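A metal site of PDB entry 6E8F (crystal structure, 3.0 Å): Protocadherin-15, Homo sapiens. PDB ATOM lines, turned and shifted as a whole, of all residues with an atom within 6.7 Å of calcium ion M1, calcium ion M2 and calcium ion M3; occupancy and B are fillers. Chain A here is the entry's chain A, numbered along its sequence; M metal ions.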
ATOM      1  N   GLU A 145      34.360  21.190 -15.602  1.00  0.00           N
ATOM      2  CA  GLU A 145      34.017  20.649 -16.931  1.00  0.00           C
ATOM      3  C   GLU A 145      34.114  21.774 -17.956  1.00  0.00           C
ATOM      4  O   GLU A 145      34.346  21.523 -19.114  1.00  0.00           O
ATOM      5  CB  GLU A 145      32.662  19.960 -16.993  1.00  0.00           C
ATOM      6  CG  GLU A 145      31.491  20.848 -16.624  1.00  0.00           C
ATOM      7  CD  GLU A 145      30.140  20.171 -16.752  1.00  0.00           C
ATOM      8  OE1 GLU A 145      30.011  19.267 -17.597  1.00  0.00           O
ATOM      9  OE2 GLU A 145      29.204  20.559 -16.029  1.00  0.00           O
ATOM     10  N   VAL A 215      36.265  17.895 -21.067  1.00  0.00           N
ATOM     11  CA  VAL A 215      35.674  16.824 -20.292  1.00  0.00           C
ATOM     12  C   VAL A 215      34.275  17.240 -19.830  1.00  0.00           C
ATOM     13  O   VAL A 215      34.059  18.358 -19.391  1.00  0.00           O
ATOM     14  CB  VAL A 215      36.571  16.452 -19.093  1.00  0.00           C
ATOM     15  CG1 VAL A 215      37.822  15.715 -19.551  1.00  0.00           C
ATOM     16  CG2 VAL A 215      36.921  17.663 -18.226  1.00  0.00           C
ATOM     17  N   ASP A 216      33.353  16.290 -19.914  1.00  0.00           N
ATOM     18  CA  ASP A 216      31.974  16.494 -19.651  1.00  0.00           C
ATOM     19  C   ASP A 216      31.629  15.777 -18.349  1.00  0.00           C
ATOM     20  O   ASP A 216      31.768  14.549 -18.262  1.00  0.00           O
ATOM     21  CB  ASP A 216      31.157  15.954 -20.825  1.00  0.00           C
ATOM     22  CG  ASP A 216      29.676  16.277 -20.791  1.00  0.00           C
ATOM     23  OD1 ASP A 216      29.184  16.772 -19.744  1.00  0.00           O
ATOM     24  OD2 ASP A 216      29.025  15.987 -21.814  1.00  0.00           O
ATOM     25  N   ARG A 217      31.186  16.532 -17.334  1.00  0.00           N
ATOM     26  CA  ARG A 217      30.843  15.888 -16.060  1.00  0.00           C
ATOM     27  C   ARG A 217      29.682  14.913 -16.274  1.00  0.00           C
ATOM     28  O   ARG A 217      29.556  13.916 -15.588  1.00  0.00           O
ATOM     29  CB  ARG A 217      30.456  16.872 -14.962  1.00  0.00           C
ATOM     30  CG  ARG A 217      30.293  16.201 -13.602  1.00  0.00           C
ATOM     31  CD  ARG A 217      29.271  16.909 -12.741  1.00  0.00           C
ATOM     32  NE  ARG A 217      27.945  16.760 -13.303  1.00  0.00           N
ATOM     33  CZ  ARG A 217      27.125  15.752 -13.006  1.00  0.00           C
ATOM     34  NH1 ARG A 217      27.557  14.773 -12.212  1.00  0.00           N
ATOM     35  NH2 ARG A 217      25.889  15.740 -13.475  1.00  0.00           N
ATOM     36  N   GLU A 218      28.824  15.220 -17.250  1.00  0.00           N
ATOM     37  CA  GLU A 218      27.627  14.436 -17.444  1.00  0.00           C
ATOM     38  C   GLU A 218      27.987  13.096 -18.106  1.00  0.00           C
ATOM     39  O   GLU A 218      27.273  12.142 -17.898  1.00  0.00           O
ATOM     40  CB  GLU A 218      26.577  15.254 -18.189  1.00  0.00           C
ATOM     41  CG  GLU A 218      25.890  16.294 -17.309  1.00  0.00           C
ATOM     42  CD  GLU A 218      26.737  17.474 -16.829  1.00  0.00           C
ATOM     43  OE1 GLU A 218      27.467  18.118 -17.673  1.00  0.00           O
ATOM     44  OE2 GLU A 218      26.656  17.760 -15.594  1.00  0.00           O
ATOM     45  N   GLU A 219      29.109  13.017 -18.857  1.00  0.00           N
ATOM     46  CA  GLU A 219      29.661  11.702 -19.285  1.00  0.00           C
ATOM     47  C   GLU A 219      30.306  10.984 -18.104  1.00  0.00           C
ATOM     48  O   GLU A 219      29.699  10.112 -17.483  1.00  0.00           O
ATOM     49  CB  GLU A 219      30.720  11.851 -20.378  1.00  0.00           C
ATOM     50  CG  GLU A 219      30.187  11.762 -21.784  1.00  0.00           C
ATOM     51  CD  GLU A 219      31.124  12.378 -22.802  1.00  0.00           C
ATOM     52  OE1 GLU A 219      30.641  12.754 -23.891  1.00  0.00           O
ATOM     53  OE2 GLU A 219      32.360  12.515 -22.481  1.00  0.00           O
ATOM     54  N   MET A 246      34.307  18.812 -11.853  1.00  0.00           N
ATOM     55  CA  MET A 246      33.347  19.596 -11.097  1.00  0.00           C
ATOM     56  C   MET A 246      32.307  20.183 -12.051  1.00  0.00           C
ATOM     57  O   MET A 246      32.623  20.585 -13.194  1.00  0.00           O
ATOM     58  CB  MET A 246      34.038  20.732 -10.350  1.00  0.00           C
ATOM     59  CG  MET A 246      35.230  20.282  -9.542  1.00  0.00           C
ATOM     60  SD  MET A 246      36.058  21.686  -8.736  1.00  0.00           S
ATOM     61  CE  MET A 246      35.307  21.594  -7.112  1.00  0.00           C
ATOM     62  N   ASP A 247      31.066  20.262 -11.545  1.00  0.00           N
ATOM     63  CA  ASP A 247      29.898  20.640 -12.307  1.00  0.00           C
ATOM     64  C   ASP A 247      29.968  22.119 -12.669  1.00  0.00           C
ATOM     65  O   ASP A 247      30.516  22.934 -11.932  1.00  0.00           O
ATOM     66  CB  ASP A 247      28.622  20.354 -11.525  1.00  0.00           C
ATOM     67  CG  ASP A 247      27.363  20.409 -12.384  1.00  0.00           C
ATOM     68  OD1 ASP A 247      27.247  19.603 -13.335  1.00  0.00           O
ATOM     69  OD2 ASP A 247      26.513  21.258 -12.090  1.00  0.00           O
ATOM     70  N   ALA A 248      29.443  22.430 -13.857  1.00  0.00           N
ATOM     71  CA  ALA A 248      29.066  23.735 -14.298  1.00  0.00           C
ATOM     72  C   ALA A 248      27.615  23.649 -14.746  1.00  0.00           C
ATOM     73  O   ALA A 248      27.124  22.542 -15.039  1.00  0.00           O
ATOM     74  CB  ALA A 248      29.960  24.150 -15.423  1.00  0.00           C
ATOM     75  N   ASN A 249      26.926  24.798 -14.811  1.00  0.00           N
ATOM     76  CA  ASN A 249      25.543  24.852 -15.256  1.00  0.00           C
ATOM     77  C   ASN A 249      25.520  24.955 -16.786  1.00  0.00           C
ATOM     78  O   ASN A 249      25.246  26.028 -17.335  1.00  0.00           O
ATOM     79  CB  ASN A 249      24.739  25.962 -14.590  1.00  0.00           C
ATOM     80  CG  ASN A 249      23.246  25.740 -14.747  1.00  0.00           C
ATOM     81  OD1 ASN A 249      22.808  24.597 -14.841  1.00  0.00           O
ATOM     82  ND2 ASN A 249      22.462  26.802 -14.772  1.00  0.00           N
ATOM     83  N   ASP A 250      25.783  23.825 -17.457  1.00  0.00           N
ATOM     84  CA  ASP A 250      25.777  23.734 -18.924  1.00  0.00           C
ATOM     85  C   ASP A 250      24.544  22.978 -19.430  1.00  0.00           C
ATOM     86  O   ASP A 250      24.496  22.556 -20.585  1.00  0.00           O
ATOM     87  CB  ASP A 250      27.070  23.111 -19.470  1.00  0.00           C
ATOM     88  CG  ASP A 250      27.622  21.873 -18.757  1.00  0.00           C
ATOM     89  OD1 ASP A 250      26.848  21.182 -18.057  1.00  0.00           O
ATOM     90  OD2 ASP A 250      28.829  21.605 -18.933  1.00  0.00           O
ATOM     91  N   ASN A 251      23.520  22.782 -18.581  1.00  0.00           N
ATOM     92  CA  ASN A 251      22.346  22.046 -18.999  1.00  0.00           C
ATOM     93  C   ASN A 251      21.081  22.787 -18.561  1.00  0.00           C
ATOM     94  O   ASN A 251      20.872  23.054 -17.371  1.00  0.00           O
ATOM     95  CB  ASN A 251      22.380  20.612 -18.479  1.00  0.00           C
ATOM     96  CG  ASN A 251      23.406  19.787 -19.228  1.00  0.00           C
ATOM     97  OD1 ASN A 251      23.093  19.229 -20.284  1.00  0.00           O
ATOM     98  ND2 ASN A 251      24.628  19.741 -18.720  1.00  0.00           N
ATOM     99  N   THR A 252      20.257  23.106 -19.569  1.00  0.00           N
ATOM    100  CA  THR A 252      19.017  23.832 -19.392  1.00  0.00           C
ATOM    101  C   THR A 252      17.943  22.840 -18.945  1.00  0.00           C
ATOM    102  O   THR A 252      17.952  21.683 -19.369  1.00  0.00           O
ATOM    103  CB  THR A 252      18.626  24.531 -20.693  1.00  0.00           C
ATOM    104  OG1 THR A 252      19.710  25.349 -21.139  1.00  0.00           O
ATOM    105  CG2 THR A 252      17.402  25.406 -20.516  1.00  0.00           C
ATOM    106  N   PRO A 253      17.011  23.237 -18.048  1.00  0.00           N
ATOM    107  CA  PRO A 253      15.876  22.376 -17.696  1.00  0.00           C
ATOM    108  C   PRO A 253      14.991  22.376 -18.940  1.00  0.00           C
ATOM    109  O   PRO A 253      14.426  23.400 -19.241  1.00  0.00           O
ATOM    110  CB  PRO A 253      15.211  23.023 -16.476  1.00  0.00           C
ATOM    111  CG  PRO A 253      16.209  24.087 -16.026  1.00  0.00           C
ATOM    112  CD  PRO A 253      17.005  24.475 -17.255  1.00  0.00           C
ATOM    113  N   ASP A 281      16.995  18.269 -15.954  1.00  0.00           N
ATOM    114  CA  ASP A 281      18.231  19.032 -15.971  1.00  0.00           C
ATOM    115  C   ASP A 281      19.318  18.072 -15.530  1.00  0.00           C
ATOM    116  O   ASP A 281      19.367  17.731 -14.354  1.00  0.00           O
ATOM    117  CB  ASP A 281      18.196  20.236 -15.023  1.00  0.00           C
ATOM    118  CG  ASP A 281      19.339  21.227 -15.206  1.00  0.00           C
ATOM    119  OD1 ASP A 281      20.487  20.793 -15.457  1.00  0.00           O
ATOM    120  OD2 ASP A 281      19.081  22.438 -15.088  1.00  0.00           O
ATOM    121  N   ALA A 282      20.177  17.676 -16.468  1.00  0.00           N
ATOM    122  CA  ALA A 282      21.194  16.641 -16.233  1.00  0.00           C
ATOM    123  C   ALA A 282      22.268  17.093 -15.223  1.00  0.00           C
ATOM    124  O   ALA A 282      22.987  16.266 -14.708  1.00  0.00           O
ATOM    125  CB  ALA A 282      21.822  16.257 -17.545  1.00  0.00           C
ATOM    126  N   ASP A 283      22.371  18.407 -14.945  1.00  0.00           N
ATOM    127  CA  ASP A 283      23.381  18.956 -14.040  1.00  0.00           C
ATOM    128  C   ASP A 283      23.279  18.330 -12.643  1.00  0.00           C
ATOM    129  O   ASP A 283      22.323  17.622 -12.323  1.00  0.00           O
ATOM    130  CB  ASP A 283      23.292  20.475 -13.993  1.00  0.00           C
ATOM    131  CG  ASP A 283      23.782  21.159 -15.266  1.00  0.00           C
ATOM    132  OD1 ASP A 283      24.692  20.591 -15.918  1.00  0.00           O
ATOM    133  OD2 ASP A 283      23.249  22.245 -15.592  1.00  0.00           O
ATOM    134  N   GLU A 284      24.307  18.610 -11.840  1.00  0.00           N
ATOM    135  CA  GLU A 284      24.498  18.076 -10.496  1.00  0.00           C
ATOM    136  C   GLU A 284      24.119  19.159  -9.491  1.00  0.00           C
ATOM    137  O   GLU A 284      24.185  20.374  -9.768  1.00  0.00           O
ATOM    138  CB  GLU A 284      25.963  17.633 -10.304  1.00  0.00           C
ATOM    139  CG  GLU A 284      26.453  17.588  -8.847  1.00  0.00           C
ATOM    140  CD  GLU A 284      27.886  17.111  -8.615  1.00  0.00           C
ATOM    141  OE1 GLU A 284      28.830  17.838  -8.984  1.00  0.00           O
ATOM    142  OE2 GLU A 284      28.051  16.011  -8.045  1.00  0.00           O
ATOM    143  N   SER A 286      22.544  21.809  -7.196  1.00  0.00           N
ATOM    144  CA  SER A 286      21.428  22.731  -7.423  1.00  0.00           C
ATOM    145  C   SER A 286      21.470  23.319  -8.849  1.00  0.00           C
ATOM    146  O   SER A 286      20.537  23.945  -9.292  1.00  0.00           O
ATOM    147  CB  SER A 286      21.389  23.783  -6.358  1.00  0.00           C
ATOM    148  OG  SER A 286      22.262  24.828  -6.696  1.00  0.00           O
ATOM    149  N   ASN A 287      22.535  23.034  -9.608  1.00  0.00           N
ATOM    150  CA  ASN A 287      22.572  23.372 -11.031  1.00  0.00           C
ATOM    151  C   ASN A 287      21.561  22.534 -11.813  1.00  0.00           C
ATOM    152  O   ASN A 287      21.214  22.893 -12.959  1.00  0.00           O
ATOM    153  CB  ASN A 287      23.959  23.153 -11.630  1.00  0.00           C
ATOM    154  CG  ASN A 287      24.991  24.103 -11.064  1.00  0.00           C
ATOM    155  OD1 ASN A 287      24.839  24.588  -9.949  1.00  0.00           O
ATOM    156  ND2 ASN A 287      26.017  24.393 -11.837  1.00  0.00           N
ATOM    157  N   GLY A 288      21.122  21.415 -11.217  1.00  0.00           N
ATOM    158  CA  GLY A 288      20.182  20.482 -11.824  1.00  0.00           C
ATOM    159  C   GLY A 288      18.881  20.380 -11.057  1.00  0.00           C
ATOM    160  O   GLY A 288      18.031  19.565 -11.398  1.00  0.00           O
ATOM    161  N   GLU A 289      18.737  21.214 -10.025  1.00  0.00           N
ATOM    162  CA  GLU A 289      17.515  21.370  -9.226  1.00  0.00           C
ATOM    163  C   GLU A 289      16.572  22.295  -9.999  1.00  0.00           C
ATOM    164  O   GLU A 289      17.004  23.334 -10.463  1.00  0.00           O
ATOM    165  CB  GLU A 289      17.920  21.950  -7.867  1.00  0.00           C
ATOM    166  CG  GLU A 289      17.016  21.620  -6.699  1.00  0.00           C
ATOM    167  CD  GLU A 289      17.060  22.716  -5.634  1.00  0.00           C
ATOM    168  OE1 GLU A 289      16.434  23.774  -5.865  1.00  0.00           O
ATOM    169  OE2 GLU A 289      17.772  22.552  -4.626  1.00  0.00           O
ATOM    170  N   ASP A 333      16.601  26.194 -13.370  1.00  0.00           N
ATOM    171  CA  ASP A 333      17.462  25.533 -12.375  1.00  0.00           C
ATOM    172  C   ASP A 333      17.794  26.529 -11.262  1.00  0.00           C
ATOM    173  O   ASP A 333      17.574  27.733 -11.437  1.00  0.00           O
ATOM    174  CB  ASP A 333      18.710  24.924 -13.027  1.00  0.00           C
ATOM    175  CG  ASP A 333      19.587  25.879 -13.822  1.00  0.00           C
ATOM    176  OD1 ASP A 333      19.616  27.095 -13.505  1.00  0.00           O
ATOM    177  OD2 ASP A 333      20.268  25.410 -14.750  1.00  0.00           O
ATOM    178  N   ASN A 334      18.316  26.043 -10.129  1.00  0.00           N
ATOM    179  CA  ASN A 334      18.644  26.885  -8.967  1.00  0.00           C
ATOM    180  C   ASN A 334      20.148  27.191  -8.918  1.00  0.00           C
ATOM    181  O   ASN A 334      20.740  27.201  -7.844  1.00  0.00           O
ATOM    182  CB  ASN A 334      18.125  26.296  -7.651  1.00  0.00           C
ATOM    183  CG  ASN A 334      16.603  26.258  -7.598  1.00  0.00           C
ATOM    184  OD1 ASN A 334      15.955  26.053  -8.618  1.00  0.00           O
ATOM    185  ND2 ASN A 334      16.026  26.478  -6.427  1.00  0.00           N
ATOM    186  N   ALA A 335      20.742  27.506 -10.069  1.00  0.00           N
ATOM    187  CA  ALA A 335      22.108  28.048 -10.087  1.00  0.00           C
ATOM    188  C   ALA A 335      22.064  29.458  -9.523  1.00  0.00           C
ATOM    189  O   ALA A 335      20.987  30.013  -9.320  1.00  0.00           O
ATOM    190  CB  ALA A 335      22.664  28.034 -11.488  1.00  0.00           C
ATOM    191  N   GLU A 339      24.278  32.717 -13.717  1.00  0.00           N
ATOM    192  CA  GLU A 339      24.654  31.487 -14.454  1.00  0.00           C
ATOM    193  C   GLU A 339      23.441  30.546 -14.626  1.00  0.00           C
ATOM    194  O   GLU A 339      23.618  29.390 -15.035  1.00  0.00           O
ATOM    195  CB  GLU A 339      25.731  30.720 -13.669  1.00  0.00           C
ATOM    196  CG  GLU A 339      26.970  31.540 -13.362  1.00  0.00           C
ATOM    197  CD  GLU A 339      27.551  31.277 -11.973  1.00  0.00           C
ATOM    198  OE1 GLU A 339      27.363  30.151 -11.453  1.00  0.00           O
ATOM    199  OE2 GLU A 339      28.156  32.209 -11.394  1.00  0.00           O
ATOM    200  N   ARG A 341      19.745  28.939 -15.860  1.00  0.00           N
ATOM    201  CA  ARG A 341      19.132  28.690 -17.153  1.00  0.00           C
ATOM    202  C   ARG A 341      17.684  28.265 -16.967  1.00  0.00           C
ATOM    203  O   ARG A 341      17.297  27.808 -15.894  1.00  0.00           O
ATOM    204  CB  ARG A 341      19.869  27.606 -17.925  1.00  0.00           C
ATOM    205  CG  ARG A 341      21.229  28.046 -18.435  1.00  0.00           C
ATOM    206  CD  ARG A 341      22.324  27.049 -18.097  1.00  0.00           C
ATOM    207  NE  ARG A 341      23.444  27.247 -19.003  1.00  0.00           N
ATOM    208  CZ  ARG A 341      23.438  26.884 -20.277  1.00  0.00           C
ATOM    209  NH1 ARG A 341      22.391  26.240 -20.762  1.00  0.00           N
ATOM    210  NH2 ARG A 341      24.460  27.174 -21.037  1.00  0.00           N
HETATM  211 CA    CA M   1      28.659  19.157 -19.683  1.00  0.00          CA
HETATM  212 CA    CA M   2      27.096  20.049 -15.665  1.00  0.00          CA
HETATM  213 CA    CA M   3      21.162  23.388 -15.208  1.00  0.00          CA
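OD1 of Asp 216 binds calcium ion M1 (2.4 Å).
Calcium ion M1 is bound by the side-chain carboxylate (OE1) of Glu 145 (2.5 Å).
The side-chain carboxylate (OE1) of Glu 218 is bound to calcium ion M1, at 2.6 Å.
OD2 of Asp 250 binds calcium ion M1, 2.6 Å away.
The guanidinium group (NE) of Arg 341 lies within hydrogen-bond range of the backbone carbonyl oxygen (O) of Asn 249 (2.7 Å).
The side-chain amide nitrogen (ND2) of Asn 249 is in hydrogen-bond range of the backbone carbonyl oxygen (O) of Glu 339 (2.8 Å).
OE1 of Glu 145 sits close to N of Arg 217, 3.0 Å away.
The backbone carbonyl oxygen (O) of Met 246 lies within hydrogen-bond range of the backbone NH (N) of Glu 145.
The side-chain amide nitrogen (ND2) of Asn 251 sits close to the side-chain carboxylate (OE1) of Glu 218 (3.4 Å).
ND2 of Asn 251 sits close to OD1 of Asp 250, 2.7 Å away.
The side-chain amide nitrogen (ND2) of Asn 287 lies within hydrogen-bond range of the side-chain carboxylate (OD2) of Asp 247.
The guanidinium group (NE) of Arg 217 sits close to the side-chain carboxylate (OD1) of Asp 247.
The side-chain carboxylate (OE2) of Glu 145 binds calcium ion M2 (2.2 Å).
OE2 of Glu 218 binds calcium ion M2, 2.3 Å away.
Calcium ion M2 is bound by OD1 of Asp 247 (2.4 Å).
OD1 of Asp 283 binds calcium ion M2.
Calcium ion M2 is bound by O of Ala 248 (2.6 Å).
Calcium ion M2 is bound by the side-chain carboxylate (OD1) of Asp 250, 2.7 Å away.
Calcium ion M2 is bound by the side-chain carboxylate (OE1) of Glu 218.
Of the 27 residues printed, 4 come within 4 Å of calcium ion M1.
Six residues have an atom within 4 Å of calcium ion M3: Asn 249, Asn 251, Asp 281, Asp 283, Asn 287 and Asp 333.
Calcium ion M3 is bound by OD1 of Asn 249 (2.1 Å), O of Asn 251 (2.2 Å), OD2 of Asp 333 (2.3 Å), OD2 of Asp 281 (2.3 Å), O of Asn 287 (2.3 Å), OD2 of Asp 283 (2.4 Å) and OD1 of Asp 281 (2.7 Å).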
